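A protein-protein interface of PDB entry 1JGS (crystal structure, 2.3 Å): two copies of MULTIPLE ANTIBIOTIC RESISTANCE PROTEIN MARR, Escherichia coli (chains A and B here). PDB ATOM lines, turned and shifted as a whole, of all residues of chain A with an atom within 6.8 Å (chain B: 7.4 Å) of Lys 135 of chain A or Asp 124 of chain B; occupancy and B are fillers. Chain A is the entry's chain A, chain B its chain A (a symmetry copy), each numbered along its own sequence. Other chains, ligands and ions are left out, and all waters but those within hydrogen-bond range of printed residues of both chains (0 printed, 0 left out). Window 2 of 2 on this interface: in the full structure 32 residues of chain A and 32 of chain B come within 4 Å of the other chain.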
ATOM      1  N   GLU A 130     -10.359 -25.987  13.864  1.00  0.00           N
ATOM      2  CA  GLU A 130      -9.476 -25.032  13.213  1.00  0.00           C
ATOM      3  C   GLU A 130      -8.532 -24.417  14.241  1.00  0.00           C
ATOM      4  O   GLU A 130      -7.341 -24.266  13.994  1.00  0.00           O
ATOM      5  CB  GLU A 130     -10.301 -23.941  12.528  1.00  0.00           C
ATOM      6  CG  GLU A 130     -11.442 -24.492  11.695  1.00  0.00           C
ATOM      7  CD  GLU A 130     -12.115 -23.444  10.824  1.00  0.00           C
ATOM      8  OE1 GLU A 130     -12.382 -22.320  11.311  1.00  0.00           O
ATOM      9  OE2 GLU A 130     -12.396 -23.759   9.645  1.00  0.00           O
ATOM     10  N   TYR A 131      -9.071 -24.081  15.403  1.00  0.00           N
ATOM     11  CA  TYR A 131      -8.282 -23.491  16.464  1.00  0.00           C
ATOM     12  C   TYR A 131      -7.135 -24.413  16.847  1.00  0.00           C
ATOM     13  O   TYR A 131      -5.970 -24.019  16.786  1.00  0.00           O
ATOM     14  CB  TYR A 131      -9.158 -23.233  17.689  1.00  0.00           C
ATOM     15  CG  TYR A 131      -8.385 -22.710  18.871  1.00  0.00           C
ATOM     16  CD1 TYR A 131      -7.923 -21.398  18.897  1.00  0.00           C
ATOM     17  CD2 TYR A 131      -8.079 -23.542  19.946  1.00  0.00           C
ATOM     18  CE1 TYR A 131      -7.171 -20.920  19.964  1.00  0.00           C
ATOM     19  CE2 TYR A 131      -7.325 -23.079  21.023  1.00  0.00           C
ATOM     20  CZ  TYR A 131      -6.873 -21.764  21.023  1.00  0.00           C
ATOM     21  OH  TYR A 131      -6.109 -21.301  22.072  1.00  0.00           O
ATOM     22  N   LEU A 132      -7.466 -25.634  17.258  1.00  0.00           N
ATOM     23  CA  LEU A 132      -6.448 -26.608  17.645  1.00  0.00           C
ATOM     24  C   LEU A 132      -5.456 -26.899  16.508  1.00  0.00           C
ATOM     25  O   LEU A 132      -4.261 -27.050  16.753  1.00  0.00           O
ATOM     26  CB  LEU A 132      -7.107 -27.913  18.106  1.00  0.00           C
ATOM     27  CG  LEU A 132      -7.872 -27.862  19.436  1.00  0.00           C
ATOM     28  CD1 LEU A 132      -8.457 -29.226  19.761  1.00  0.00           C
ATOM     29  CD2 LEU A 132      -6.925 -27.431  20.536  1.00  0.00           C
ATOM     30  N   LEU A 133      -5.942 -26.970  15.271  1.00  0.00           N
ATOM     31  CA  LEU A 133      -5.057 -27.239  14.144  1.00  0.00           C
ATOM     32  C   LEU A 133      -4.045 -26.117  13.972  1.00  0.00           C
ATOM     33  O   LEU A 133      -2.957 -26.331  13.441  1.00  0.00           O
ATOM     34  CB  LEU A 133      -5.860 -27.410  12.849  1.00  0.00           C
ATOM     35  CG  LEU A 133      -6.522 -28.772  12.603  1.00  0.00           C
ATOM     36  CD1 LEU A 133      -7.337 -28.707  11.313  1.00  0.00           C
ATOM     37  CD2 LEU A 133      -5.462 -29.863  12.512  1.00  0.00           C
ATOM     38  N   LYS A 134      -4.405 -24.915  14.408  1.00  0.00           N
ATOM     39  CA  LYS A 134      -3.490 -23.783  14.298  1.00  0.00           C
ATOM     40  C   LYS A 134      -2.387 -23.934  15.327  1.00  0.00           C
ATOM     41  O   LYS A 134      -1.225 -23.655  15.038  1.00  0.00           O
ATOM     42  CB  LYS A 134      -4.222 -22.454  14.513  1.00  0.00           C
ATOM     43  CG  LYS A 134      -5.140 -22.059  13.363  1.00  0.00           C
ATOM     44  CD  LYS A 134      -5.802 -20.709  13.609  1.00  0.00           C
ATOM     45  CE  LYS A 134      -6.642 -20.276  12.419  1.00  0.00           C
ATOM     46  NZ  LYS A 134      -7.172 -18.888  12.595  1.00  0.00           N
ATOM     47  N   LYS A 135      -2.753 -24.391  16.523  1.00  0.00           N
ATOM     48  CA  LYS A 135      -1.785 -24.580  17.598  1.00  0.00           C
ATOM     49  C   LYS A 135      -0.725 -25.613  17.240  1.00  0.00           C
ATOM     50  O   LYS A 135       0.244 -25.799  17.977  1.00  0.00           O
ATOM     51  CB  LYS A 135      -2.485 -24.990  18.902  1.00  0.00           C
ATOM     52  CG  LYS A 135      -3.411 -23.930  19.475  1.00  0.00           C
ATOM     53  CD  LYS A 135      -3.650 -24.134  20.967  1.00  0.00           C
ATOM     54  CE  LYS A 135      -2.396 -23.790  21.783  1.00  0.00           C
ATOM     55  NZ  LYS A 135      -2.548 -23.992  23.267  1.00  0.00           N
ATOM     56  N   VAL A 136      -0.905 -26.283  16.107  1.00  0.00           N
ATOM     57  CA  VAL A 136       0.053 -27.280  15.647  1.00  0.00           C
ATOM     58  C   VAL A 136       1.095 -26.661  14.702  1.00  0.00           C
ATOM     59  O   VAL A 136       2.222 -27.148  14.610  1.00  0.00           O
ATOM     60  CB  VAL A 136      -0.659 -28.436  14.892  1.00  0.00           C
ATOM     61  CG1 VAL A 136       0.370 -29.349  14.246  1.00  0.00           C
ATOM     62  CG2 VAL A 136      -1.542 -29.228  15.848  1.00  0.00           C
ATOM     63  N   LEU A 137       0.725 -25.580  14.020  1.00  0.00           N
ATOM     64  CA  LEU A 137       1.616 -24.934  13.055  1.00  0.00           C
ATOM     65  C   LEU A 137       2.858 -24.173  13.553  1.00  0.00           C
ATOM     66  O   LEU A 137       3.969 -24.379  13.045  1.00  0.00           O
ATOM     67  CB  LEU A 137       0.790 -24.021  12.138  1.00  0.00           C
ATOM     68  CG  LEU A 137      -0.125 -24.813  11.206  1.00  0.00           C
ATOM     69  CD1 LEU A 137      -0.878 -23.889  10.289  1.00  0.00           C
ATOM     70  CD2 LEU A 137       0.715 -25.790  10.412  1.00  0.00           C
ATOM     71  N   PRO A 138       2.699 -23.285  14.542  1.00  0.00           N
ATOM     72  CA  PRO A 138       3.888 -22.563  15.005  1.00  0.00           C
ATOM     73  C   PRO A 138       4.978 -23.469  15.603  1.00  0.00           C
ATOM     74  O   PRO A 138       4.673 -24.622  15.973  1.00  0.00           O
ATOM     75  CB  PRO A 138       3.312 -21.579  16.025  1.00  0.00           C
ATOM     76  CG  PRO A 138       2.137 -22.326  16.580  1.00  0.00           C
ATOM     77  CD  PRO A 138       1.516 -22.932  15.345  1.00  0.00           C
ATOM     78  OXT PRO A 138       6.131 -23.005  15.702  1.00  0.00           O
ATOM     79  N   LEU B   1      -2.033 -15.274  13.119  1.00  0.00           N
ATOM     80  CA  LEU B   1      -2.479 -16.634  12.703  1.00  0.00           C
ATOM     81  C   LEU B   1      -3.802 -16.951  13.385  1.00  0.00           C
ATOM     82  O   LEU B   1      -4.701 -17.535  12.774  1.00  0.00           O
ATOM     83  CB  LEU B   1      -1.426 -17.683  13.083  1.00  0.00           C
ATOM     84  CG  LEU B   1      -1.486 -19.036  12.360  1.00  0.00           C
ATOM     85  CD1 LEU B   1      -1.254 -18.831  10.879  1.00  0.00           C
ATOM     86  CD2 LEU B   1      -0.434 -19.985  12.925  1.00  0.00           C
ATOM     87  N   PHE B   2      -3.921 -16.568  14.655  1.00  0.00           N
ATOM     88  CA  PHE B   2      -5.151 -16.798  15.411  1.00  0.00           C
ATOM     89  C   PHE B   2      -6.061 -15.585  15.292  1.00  0.00           C
ATOM     90  O   PHE B   2      -7.048 -15.461  16.014  1.00  0.00           O
ATOM     91  CB  PHE B   2      -4.851 -17.067  16.889  1.00  0.00           C
ATOM     92  CG  PHE B   2      -4.215 -18.405  17.148  1.00  0.00           C
ATOM     93  CD1 PHE B   2      -2.907 -18.666  16.737  1.00  0.00           C
ATOM     94  CD2 PHE B   2      -4.925 -19.411  17.799  1.00  0.00           C
ATOM     95  CE1 PHE B   2      -2.317 -19.906  16.971  1.00  0.00           C
ATOM     96  CE2 PHE B   2      -4.342 -20.658  18.037  1.00  0.00           C
ATOM     97  CZ  PHE B   2      -3.037 -20.903  17.623  1.00  0.00           C
ATOM     98  N   VAL B  15      -1.018 -28.205   7.668  1.00  0.00           N
ATOM     99  CA  VAL B  15      -0.579 -29.136   8.706  1.00  0.00           C
ATOM    100  C   VAL B  15       0.025 -30.420   8.136  1.00  0.00           C
ATOM    101  O   VAL B  15       0.984 -30.978   8.700  1.00  0.00           O
ATOM    102  CB  VAL B  15      -1.734 -29.528   9.652  1.00  0.00           C
ATOM    103  CG1 VAL B  15      -1.224 -30.517  10.692  1.00  0.00           C
ATOM    104  CG2 VAL B  15      -2.299 -28.272  10.350  1.00  0.00           C
ATOM    105  N   LYS B  18       3.450 -29.407   6.977  1.00  0.00           N
ATOM    106  CA  LYS B  18       4.359 -29.432   8.114  1.00  0.00           C
ATOM    107  C   LYS B  18       4.770 -30.856   8.452  1.00  0.00           C
ATOM    108  O   LYS B  18       5.954 -31.154   8.587  1.00  0.00           O
ATOM    109  CB  LYS B  18       3.705 -28.798   9.347  1.00  0.00           C
ATOM    110  CG  LYS B  18       4.652 -28.708  10.534  1.00  0.00           C
ATOM    111  CD  LYS B  18       3.927 -28.444  11.838  1.00  0.00           C
ATOM    112  CE  LYS B  18       4.902 -28.341  13.019  1.00  0.00           C
ATOM    113  NZ  LYS B  18       5.323 -26.935  13.315  1.00  0.00           N
ATOM    114  N   GLU B 116       6.778 -33.590  18.331  1.00  0.00           N
ATOM    115  CA  GLU B 116       6.811 -32.312  17.628  1.00  0.00           C
ATOM    116  C   GLU B 116       5.448 -31.712  17.321  1.00  0.00           C
ATOM    117  O   GLU B 116       5.236 -30.516  17.537  1.00  0.00           O
ATOM    118  CB  GLU B 116       7.613 -32.435  16.332  1.00  0.00           C
ATOM    119  CG  GLU B 116       9.118 -32.354  16.526  1.00  0.00           C
ATOM    120  CD  GLU B 116       9.525 -31.157  17.361  1.00  0.00           C
ATOM    121  OE1 GLU B 116       9.507 -31.269  18.606  1.00  0.00           O
ATOM    122  OE2 GLU B 116       9.847 -30.103  16.772  1.00  0.00           O
ATOM    123  N   LEU B 117       4.530 -32.531  16.815  1.00  0.00           N
ATOM    124  CA  LEU B 117       3.187 -32.068  16.476  1.00  0.00           C
ATOM    125  C   LEU B 117       2.405 -31.670  17.718  1.00  0.00           C
ATOM    126  O   LEU B 117       1.651 -30.693  17.717  1.00  0.00           O
ATOM    127  CB  LEU B 117       2.405 -33.169  15.747  1.00  0.00           C
ATOM    128  CG  LEU B 117       2.878 -33.622  14.368  1.00  0.00           C
ATOM    129  CD1 LEU B 117       1.987 -34.750  13.864  1.00  0.00           C
ATOM    130  CD2 LEU B 117       2.845 -32.433  13.419  1.00  0.00           C
ATOM    131  N   THR B 118       2.594 -32.449  18.774  1.00  0.00           N
ATOM    132  CA  THR B 118       1.909 -32.245  20.042  1.00  0.00           C
ATOM    133  C   THR B 118       2.687 -31.336  20.989  1.00  0.00           C
ATOM    134  O   THR B 118       2.195 -30.993  22.055  1.00  0.00           O
ATOM    135  CB  THR B 118       1.661 -33.626  20.718  1.00  0.00           C
ATOM    136  OG1 THR B 118       0.524 -34.253  20.111  1.00  0.00           O
ATOM    137  CG2 THR B 118       1.439 -33.493  22.208  1.00  0.00           C
ATOM    138  N   LYS B 119       3.889 -30.929  20.583  1.00  0.00           N
ATOM    139  CA  LYS B 119       4.752 -30.094  21.421  1.00  0.00           C
ATOM    140  C   LYS B 119       4.075 -28.914  22.116  1.00  0.00           C
ATOM    141  O   LYS B 119       4.414 -28.591  23.255  1.00  0.00           O
ATOM    142  CB  LYS B 119       5.944 -29.565  20.614  1.00  0.00           C
ATOM    143  CG  LYS B 119       5.606 -28.447  19.629  1.00  0.00           C
ATOM    144  CD  LYS B 119       6.877 -27.849  19.028  1.00  0.00           C
ATOM    145  CE  LYS B 119       6.583 -26.760  18.003  1.00  0.00           C
ATOM    146  NZ  LYS B 119       7.843 -26.200  17.433  1.00  0.00           N
ATOM    147  N   ASN B 120       3.125 -28.268  21.443  1.00  0.00           N
ATOM    148  CA  ASN B 120       2.464 -27.121  22.044  1.00  0.00           C
ATOM    149  C   ASN B 120       0.955 -27.160  22.231  1.00  0.00           C
ATOM    150  O   ASN B 120       0.406 -26.305  22.917  1.00  0.00           O
ATOM    151  CB  ASN B 120       2.860 -25.837  21.295  1.00  0.00           C
ATOM    152  CG  ASN B 120       2.853 -26.002  19.786  1.00  0.00           C
ATOM    153  OD1 ASN B 120       3.283 -25.106  19.054  1.00  0.00           O
ATOM    154  ND2 ASN B 120       2.365 -27.146  19.313  1.00  0.00           N
ATOM    155  N   LEU B 121       0.257 -28.129  21.662  1.00  0.00           N
ATOM    156  CA  LEU B 121      -1.180 -28.129  21.879  1.00  0.00           C
ATOM    157  C   LEU B 121      -1.564 -29.057  23.031  1.00  0.00           C
ATOM    158  O   LEU B 121      -2.696 -29.013  23.514  1.00  0.00           O
ATOM    159  CB  LEU B 121      -1.926 -28.508  20.591  1.00  0.00           C
ATOM    160  CG  LEU B 121      -2.144 -29.967  20.202  1.00  0.00           C
ATOM    161  CD1 LEU B 121      -3.064 -30.664  21.207  1.00  0.00           C
ATOM    162  CD2 LEU B 121      -2.781 -30.009  18.825  1.00  0.00           C
ATOM    163  N   THR B 122      -0.611 -29.874  23.478  1.00  0.00           N
ATOM    164  CA  THR B 122      -0.830 -30.836  24.565  1.00  0.00           C
ATOM    165  C   THR B 122      -1.813 -30.377  25.647  1.00  0.00           C
ATOM    166  O   THR B 122      -2.639 -31.163  26.123  1.00  0.00           O
ATOM    167  CB  THR B 122       0.498 -31.216  25.263  1.00  0.00           C
ATOM    168  OG1 THR B 122       1.444 -31.673  24.289  1.00  0.00           O
ATOM    169  CG2 THR B 122       0.263 -32.334  26.276  1.00  0.00           C
ATOM    170  N   ALA B 123      -1.713 -29.115  26.048  1.00  0.00           N
ATOM    171  CA  ALA B 123      -2.610 -28.575  27.059  1.00  0.00           C
ATOM    172  C   ALA B 123      -4.037 -28.759  26.560  1.00  0.00           C
ATOM    173  O   ALA B 123      -4.850 -29.425  27.206  1.00  0.00           O
ATOM    174  CB  ALA B 123      -2.320 -27.098  27.287  1.00  0.00           C
ATOM    175  N   ASP B 124      -4.345 -28.132  25.420  1.00  0.00           N
ATOM    176  CA  ASP B 124      -5.655 -28.268  24.786  1.00  0.00           C
ATOM    177  C   ASP B 124      -5.975 -29.741  24.618  1.00  0.00           C
ATOM    178  O   ASP B 124      -7.145 -30.136  24.484  1.00  0.00           O
ATOM    179  CB  ASP B 124      -5.667 -27.587  23.413  1.00  0.00           C
ATOM    180  CG  ASP B 124      -5.075 -26.189  23.499  1.00  0.00           C
ATOM    181  OD1 ASP B 124      -3.903 -26.050  23.911  1.00  0.00           O
ATOM    182  OD2 ASP B 124      -5.802 -25.236  23.150  1.00  0.00           O
ATOM    183  N   GLU B 125      -4.911 -30.581  24.595  1.00  0.00           N
ATOM    184  CA  GLU B 125      -4.988 -32.083  24.617  1.00  0.00           C
ATOM    185  C   GLU B 125      -5.174 -32.871  23.328  1.00  0.00           C
ATOM    186  O   GLU B 125      -6.296 -32.969  22.824  1.00  0.00           O
ATOM    187  CB  GLU B 125      -6.121 -32.464  25.541  1.00  0.00           C
ATOM    188  CG  GLU B 125      -5.982 -33.918  25.886  1.00  0.00           C
ATOM    189  CD  GLU B 125      -4.582 -34.178  26.369  1.00  0.00           C
ATOM    190  OE1 GLU B 125      -3.918 -35.113  25.857  1.00  0.00           O
ATOM    191  OE2 GLU B 125      -4.118 -33.444  27.258  1.00  0.00           O
ATOM    192  N   VAL B 126      -4.115 -33.461  22.734  1.00  0.00           N
ATOM    193  CA  VAL B 126      -4.180 -34.170  21.418  1.00  0.00           C
ATOM    194  C   VAL B 126      -5.437 -35.025  21.190  1.00  0.00           C
ATOM    195  O   VAL B 126      -5.868 -35.237  20.070  1.00  0.00           O
ATOM    196  CB  VAL B 126      -2.902 -35.001  21.242  1.00  0.00           C
ATOM    197  CG1 VAL B 126      -2.696 -35.396  19.787  1.00  0.00           C
ATOM    198  CG2 VAL B 126      -1.699 -34.230  21.752  1.00  0.00           C
ATOM    199  N   ALA B 127      -5.958 -35.504  22.304  1.00  0.00           N
ATOM    200  CA  ALA B 127      -7.151 -36.342  22.326  1.00  0.00           C
ATOM    201  C   ALA B 127      -8.373 -35.602  21.775  1.00  0.00           C
ATOM    202  O   ALA B 127      -9.221 -36.207  21.124  1.00  0.00           O
ATOM    203  CB  ALA B 127      -7.437 -36.842  23.733  1.00  0.00           C
ATOM    204  N   THR B 128      -8.471 -34.303  22.040  1.00  0.00           N
ATOM    205  CA  THR B 128      -9.592 -33.507  21.543  1.00  0.00           C
ATOM    206  C   THR B 128      -9.472 -33.291  20.028  1.00  0.00           C
ATOM    207  O   THR B 128     -10.437 -33.469  19.285  1.00  0.00           O
ATOM    208  CB  THR B 128      -9.631 -32.142  22.243  1.00  0.00           C
ATOM    209  OG1 THR B 128      -9.615 -32.352  23.662  1.00  0.00           O
ATOM    210  CG2 THR B 128     -10.886 -31.356  21.855  1.00  0.00           C
ATOM    211  N   LEU B 129      -8.286 -32.898  19.574  1.00  0.00           N
ATOM    212  CA  LEU B 129      -8.062 -32.691  18.154  1.00  0.00           C
ATOM    213  C   LEU B 129      -8.316 -34.015  17.451  1.00  0.00           C
ATOM    214  O   LEU B 129      -8.980 -34.067  16.415  1.00  0.00           O
ATOM    215  CB  LEU B 129      -6.626 -32.240  17.897  1.00  0.00           C
ATOM    216  CG  LEU B 129      -6.207 -32.032  16.421  1.00  0.00           C
ATOM    217  CD1 LEU B 129      -7.149 -31.056  15.725  1.00  0.00           C
ATOM    218  CD2 LEU B 129      -4.766 -31.515  16.381  1.00  0.00           C
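Of the 9 printed residues of chain A, 8 touch a printed residue of chain B. Of the 18 printed residues of chain B, 11 touch a printed residue of chain A.
Of the printed residues of chain B, Tyr 131 of chain A touches Phe 2 and Asp 124. Of the printed residues of chain B, Lys 135 of chain A touches Phe 2 (3.6 Å), Asn 120 (2.8 Å), Leu 121 (3.9 Å) and Asp 124 (2.5 Å). Of the printed residues of chain A, Leu 1 of chain B touches Lys 134. Of the printed residues of chain A, Val 15 of chain B touches Leu 133 (3.7 Å) and Leu 137 (3.9 Å). Thr 118 of chain B touches none of the printed residues of chain A. Of chain A, only Tyr 131 (3.4 Å), Leu 132 (3.1 Å) and Lys 135 (2.5 Å) come within 4 Å of Asp 124 of chain B. Ala 127 of chain B touches none of the printed residues of chain A. The nearest printed residue of chain B that does not touch Lys 135 of chain A is Ala 123 of chain B (5.1 Å).
NZ of Lys 18 of chain B lies within salt-bridge range of O of Pro 138 of chain A, 3.6 Å away. O of Pro 138 of chain A lies close to OD1 of Asn 120 of chain B (3.4 Å). The side-chain amino group (NZ) of Lys 18 of chain B sits close to the backbone carbonyl oxygen (O) of Val 136 of chain A (3.4 Å). NZ of Lys 119 of chain B is in salt-bridge range of O of Pro 138 of chain A, at 3.8 Å. The side-chain carboxylate (OD1) of Asp 124 of chain B is in salt-bridge range of the side-chain amino group (NZ) of Lys 135 of chain A, 2.5 Å away. ND2 of Asn 120 of chain B sits at hydrogen-bond distance from O of Lys 135 of chain A, at 2.8 Å. O of Leu 137 of chain A sits at hydrogen-bond distance from NZ of Lys 18 of chain B, at 2.9 Å. O of Leu 1 of chain B is in hydrogen-bond range of NZ of Lys 134 of chain A, 2.8 Å away.
The side-chain hydroxyl of Thr 128 of chain B sits at hydrogen-bond distance from the backbone carbonyl oxygen of Asp 124 of chain B, at 3.4 Å. OG1 of Thr 128 of chain B lies within hydrogen-bond range of O of Glu 125 of chain B (3.5 Å).
Among the printed residues, merely in contact across the chains: Leu 132 of chain A with Asp 124 of chain B, Val 136 of chain A with Leu 121 of chain B, Tyr 131 of chain A with Asp 124 of chain B, Tyr 131 of chain A with Phe 2 of chain B, Lys 135 of chain A with Phe 2 of chain B, Lys 134 of chain A with Phe 2 of chain B, Leu 132 of chain A with Leu 129 of chain B, Leu 133 of chain A with Val 15 of chain B, Leu 133 of chain A with Leu 129 of chain B, Leu 132 of chain A with Thr 128 of chain B, Leu 132 of chain A with Leu 121 of chain B, Leu 137 of chain A with Val 15 of chain B, Val 136 of chain A with Leu 117 of chain B, Lys 135 of chain A with Leu 121 of chain B and Val 136 of chain A with Leu 129 of chain B.
No position is printed for both chains. Of the 23 pairs that touch across the chains among the printed residues, none has its exchanged pair printed and touching as well.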
